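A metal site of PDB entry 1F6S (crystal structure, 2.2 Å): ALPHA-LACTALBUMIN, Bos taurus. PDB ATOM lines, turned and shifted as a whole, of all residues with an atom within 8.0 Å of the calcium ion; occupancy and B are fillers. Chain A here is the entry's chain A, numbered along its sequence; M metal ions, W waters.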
ATOM      1  N   THR A  38      16.783 -22.206 -20.186  1.00  0.00           N
ATOM      2  CA  THR A  38      18.014 -22.566 -20.868  1.00  0.00           C
ATOM      3  C   THR A  38      18.705 -21.360 -21.513  1.00  0.00           C
ATOM      4  O   THR A  38      19.857 -21.471 -21.943  1.00  0.00           O
ATOM      5  CB  THR A  38      17.795 -23.622 -21.965  1.00  0.00           C
ATOM      6  OG1 THR A  38      16.889 -23.106 -22.939  1.00  0.00           O
ATOM      7  CG2 THR A  38      17.222 -24.906 -21.347  1.00  0.00           C
ATOM      8  N   ILE A  75      34.776 -25.294 -25.039  1.00  0.00           N
ATOM      9  CA  ILE A  75      33.574 -25.033 -25.782  1.00  0.00           C
ATOM     10  C   ILE A  75      33.219 -23.566 -25.674  1.00  0.00           C
ATOM     11  O   ILE A  75      33.572 -22.901 -24.698  1.00  0.00           O
ATOM     12  CB  ILE A  75      32.413 -25.890 -25.226  1.00  0.00           C
ATOM     13  CG1 ILE A  75      31.237 -25.879 -26.182  1.00  0.00           C
ATOM     14  CG2 ILE A  75      31.975 -25.361 -23.874  1.00  0.00           C
ATOM     15  CD1 ILE A  75      30.177 -26.908 -25.797  1.00  0.00           C
ATOM     16  N   SER A  76      32.543 -23.061 -26.698  1.00  0.00           N
ATOM     17  CA  SER A  76      32.140 -21.663 -26.691  1.00  0.00           C
ATOM     18  C   SER A  76      30.890 -21.594 -25.822  1.00  0.00           C
ATOM     19  O   SER A  76      30.005 -22.435 -25.924  1.00  0.00           O
ATOM     20  CB  SER A  76      31.822 -21.213 -28.120  1.00  0.00           C
ATOM     21  OG  SER A  76      31.859 -19.801 -28.185  1.00  0.00           O
ATOM     22  N   CYS A  77      30.839 -20.592 -24.960  1.00  0.00           N
ATOM     23  CA  CYS A  77      29.721 -20.429 -24.040  1.00  0.00           C
ATOM     24  C   CYS A  77      28.338 -20.386 -24.694  1.00  0.00           C
ATOM     25  O   CYS A  77      27.358 -20.853 -24.108  1.00  0.00           O
ATOM     26  CB  CYS A  77      29.911 -19.161 -23.210  1.00  0.00           C
ATOM     27  SG  CYS A  77      31.433 -19.097 -22.201  1.00  0.00           S
ATOM     28  N   ASP A  78      28.261 -19.831 -25.899  1.00  0.00           N
ATOM     29  CA  ASP A  78      26.971 -19.731 -26.578  1.00  0.00           C
ATOM     30  C   ASP A  78      26.326 -21.110 -26.756  1.00  0.00           C
ATOM     31  O   ASP A  78      25.112 -21.199 -26.917  1.00  0.00           O
ATOM     32  CB  ASP A  78      27.131 -19.044 -27.937  1.00  0.00           C
ATOM     33  CG  ASP A  78      28.095 -19.763 -28.850  1.00  0.00           C
ATOM     34  OD1 ASP A  78      29.318 -19.667 -28.613  1.00  0.00           O
ATOM     35  OD2 ASP A  78      27.634 -20.445 -29.796  1.00  0.00           O
ATOM     36  N   LYS A  79      27.129 -22.169 -26.716  1.00  0.00           N
ATOM     37  CA  LYS A  79      26.593 -23.521 -26.864  1.00  0.00           C
ATOM     38  C   LYS A  79      25.745 -23.914 -25.652  1.00  0.00           C
ATOM     39  O   LYS A  79      25.088 -24.949 -25.664  1.00  0.00           O
ATOM     40  CB  LYS A  79      27.720 -24.532 -27.035  1.00  0.00           C
ATOM     41  CG  LYS A  79      28.430 -24.458 -28.367  1.00  0.00           C
ATOM     42  CD  LYS A  79      27.512 -24.896 -29.483  1.00  0.00           C
ATOM     43  CE  LYS A  79      28.168 -24.695 -30.834  1.00  0.00           C
ATOM     44  NZ  LYS A  79      27.349 -25.321 -31.907  1.00  0.00           N
ATOM     45  N   PHE A  80      25.778 -23.084 -24.613  1.00  0.00           N
ATOM     46  CA  PHE A  80      25.032 -23.353 -23.398  1.00  0.00           C
ATOM     47  C   PHE A  80      23.675 -22.634 -23.363  1.00  0.00           C
ATOM     48  O   PHE A  80      22.991 -22.669 -22.343  1.00  0.00           O
ATOM     49  CB  PHE A  80      25.865 -22.942 -22.175  1.00  0.00           C
ATOM     50  CG  PHE A  80      27.083 -23.803 -21.960  1.00  0.00           C
ATOM     51  CD1 PHE A  80      28.221 -23.269 -21.369  1.00  0.00           C
ATOM     52  CD2 PHE A  80      27.087 -25.143 -22.311  1.00  0.00           C
ATOM     53  CE1 PHE A  80      29.342 -24.063 -21.128  1.00  0.00           C
ATOM     54  CE2 PHE A  80      28.205 -25.951 -22.070  1.00  0.00           C
ATOM     55  CZ  PHE A  80      29.329 -25.400 -21.481  1.00  0.00           C
ATOM     56  N   LEU A  81      23.289 -22.013 -24.468  1.00  0.00           N
ATOM     57  CA  LEU A  81      22.032 -21.290 -24.551  1.00  0.00           C
ATOM     58  C   LEU A  81      20.978 -21.918 -25.472  1.00  0.00           C
ATOM     59  O   LEU A  81      19.893 -21.361 -25.624  1.00  0.00           O
ATOM     60  CB  LEU A  81      22.286 -19.843 -24.992  1.00  0.00           C
ATOM     61  CG  LEU A  81      23.178 -19.004 -24.056  1.00  0.00           C
ATOM     62  CD1 LEU A  81      23.562 -17.701 -24.745  1.00  0.00           C
ATOM     63  CD2 LEU A  81      22.448 -18.742 -22.737  1.00  0.00           C
ATOM     64  N   ASP A  82      21.283 -23.059 -26.089  1.00  0.00           N
ATOM     65  CA  ASP A  82      20.311 -23.705 -26.974  1.00  0.00           C
ATOM     66  C   ASP A  82      19.512 -24.766 -26.239  1.00  0.00           C
ATOM     67  O   ASP A  82      19.684 -24.942 -25.042  1.00  0.00           O
ATOM     68  CB  ASP A  82      20.974 -24.322 -28.194  1.00  0.00           C
ATOM     69  CG  ASP A  82      22.097 -25.269 -27.844  1.00  0.00           C
ATOM     70  OD1 ASP A  82      22.076 -25.842 -26.728  1.00  0.00           O
ATOM     71  OD2 ASP A  82      23.004 -25.433 -28.691  1.00  0.00           O
ATOM     72  N   ASP A  83      18.657 -25.489 -26.971  1.00  0.00           N
ATOM     73  CA  ASP A  83      17.801 -26.502 -26.357  1.00  0.00           C
ATOM     74  C   ASP A  83      18.435 -27.853 -26.111  1.00  0.00           C
ATOM     75  O   ASP A  83      17.871 -28.689 -25.411  1.00  0.00           O
ATOM     76  CB  ASP A  83      16.523 -26.698 -27.172  1.00  0.00           C
ATOM     77  CG  ASP A  83      15.699 -25.432 -27.326  1.00  0.00           C
ATOM     78  OD1 ASP A  83      15.657 -24.618 -26.376  1.00  0.00           O
ATOM     79  OD2 ASP A  83      15.080 -25.274 -28.402  1.00  0.00           O
ATOM     80  N   ASP A  84      19.599 -28.099 -26.694  1.00  0.00           N
ATOM     81  CA  ASP A  84      20.269 -29.373 -26.509  1.00  0.00           C
ATOM     82  C   ASP A  84      21.240 -29.304 -25.323  1.00  0.00           C
ATOM     83  O   ASP A  84      22.300 -28.670 -25.412  1.00  0.00           O
ATOM     84  CB  ASP A  84      21.006 -29.771 -27.775  1.00  0.00           C
ATOM     85  CG  ASP A  84      21.925 -30.943 -27.562  1.00  0.00           C
ATOM     86  OD1 ASP A  84      21.520 -31.890 -26.848  1.00  0.00           O
ATOM     87  OD2 ASP A  84      23.036 -30.922 -28.108  1.00  0.00           O
ATOM     88  N   LEU A  85      20.870 -29.967 -24.228  1.00  0.00           N
ATOM     89  CA  LEU A  85      21.664 -29.954 -22.995  1.00  0.00           C
ATOM     90  C   LEU A  85      22.815 -30.951 -22.928  1.00  0.00           C
ATOM     91  O   LEU A  85      23.485 -31.059 -21.891  1.00  0.00           O
ATOM     92  CB  LEU A  85      20.726 -30.155 -21.797  1.00  0.00           C
ATOM     93  CG  LEU A  85      19.599 -29.129 -21.736  1.00  0.00           C
ATOM     94  CD1 LEU A  85      18.658 -29.428 -20.575  1.00  0.00           C
ATOM     95  CD2 LEU A  85      20.190 -27.751 -21.599  1.00  0.00           C
ATOM     96  N   THR A  86      23.056 -31.663 -24.018  1.00  0.00           N
ATOM     97  CA  THR A  86      24.122 -32.657 -24.066  1.00  0.00           C
ATOM     98  C   THR A  86      25.492 -32.082 -23.766  1.00  0.00           C
ATOM     99  O   THR A  86      26.229 -32.620 -22.937  1.00  0.00           O
ATOM    100  CB  THR A  86      24.151 -33.360 -25.421  1.00  0.00           C
ATOM    101  OG1 THR A  86      22.851 -33.894 -25.693  1.00  0.00           O
ATOM    102  CG2 THR A  86      25.168 -34.495 -25.399  1.00  0.00           C
ATOM    103  N   ASP A  87      25.876 -31.003 -24.436  1.00  0.00           N
ATOM    104  CA  ASP A  87      27.184 -30.435 -24.174  1.00  0.00           C
ATOM    105  C   ASP A  87      27.230 -29.739 -22.812  1.00  0.00           C
ATOM    106  O   ASP A  87      28.285 -29.721 -22.153  1.00  0.00           O
ATOM    107  CB  ASP A  87      27.645 -29.483 -25.301  1.00  0.00           C
ATOM    108  CG  ASP A  87      26.551 -28.514 -25.742  1.00  0.00           C
ATOM    109  OD1 ASP A  87      25.519 -28.401 -25.055  1.00  0.00           O
ATOM    110  OD2 ASP A  87      26.753 -27.851 -26.786  1.00  0.00           O
ATOM    111  N   ASP A  88      26.083 -29.183 -22.379  1.00  0.00           N
ATOM    112  CA  ASP A  88      26.004 -28.524 -21.073  1.00  0.00           C
ATOM    113  C   ASP A  88      26.320 -29.571 -19.992  1.00  0.00           C
ATOM    114  O   ASP A  88      27.130 -29.355 -19.107  1.00  0.00           O
ATOM    115  CB  ASP A  88      24.590 -27.985 -20.790  1.00  0.00           C
ATOM    116  CG  ASP A  88      24.099 -26.987 -21.836  1.00  0.00           C
ATOM    117  OD1 ASP A  88      23.983 -27.373 -23.009  1.00  0.00           O
ATOM    118  OD2 ASP A  88      23.799 -25.837 -21.470  1.00  0.00           O
ATOM    119  N   ILE A  89      25.657 -30.721 -20.088  1.00  0.00           N
ATOM    120  CA  ILE A  89      25.846 -31.806 -19.142  1.00  0.00           C
ATOM    121  C   ILE A  89      27.273 -32.354 -19.127  1.00  0.00           C
ATOM    122  O   ILE A  89      27.795 -32.681 -18.063  1.00  0.00           O
ATOM    123  CB  ILE A  89      24.837 -32.907 -19.417  1.00  0.00           C
ATOM    124  CG1 ILE A  89      23.466 -32.427 -18.928  1.00  0.00           C
ATOM    125  CG2 ILE A  89      25.262 -34.219 -18.753  1.00  0.00           C
ATOM    126  CD1 ILE A  89      22.289 -33.117 -19.560  1.00  0.00           C
HETATM  127 CA    CA M   1      23.745 -26.850 -25.361  1.00  0.00          CA
HETATM  128  O   HOH W   1      24.451 -27.559 -27.739  1.00  0.00           O
HETATM  129  O   HOH W   2      22.038 -25.473 -23.997  1.00  0.00           O
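The side-chain carboxylate of Asp 84 is in hydrogen-bond range of the side-chain hydroxyl of Thr 86 (2.7 Å).
The calcium ion is bound by O of Asp 84, O of Lys 79, OD1 of Asp 87, OD1 of Asp 82, OD1 of Asp 88, water W1 and water W2.
Water W1 lies within hydrogen-bond range of the side-chain carboxylate (OD2) of Asp 87 (2.5 Å) and the side-chain carboxylate (OD2) of Asp 82 (2.7 Å).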
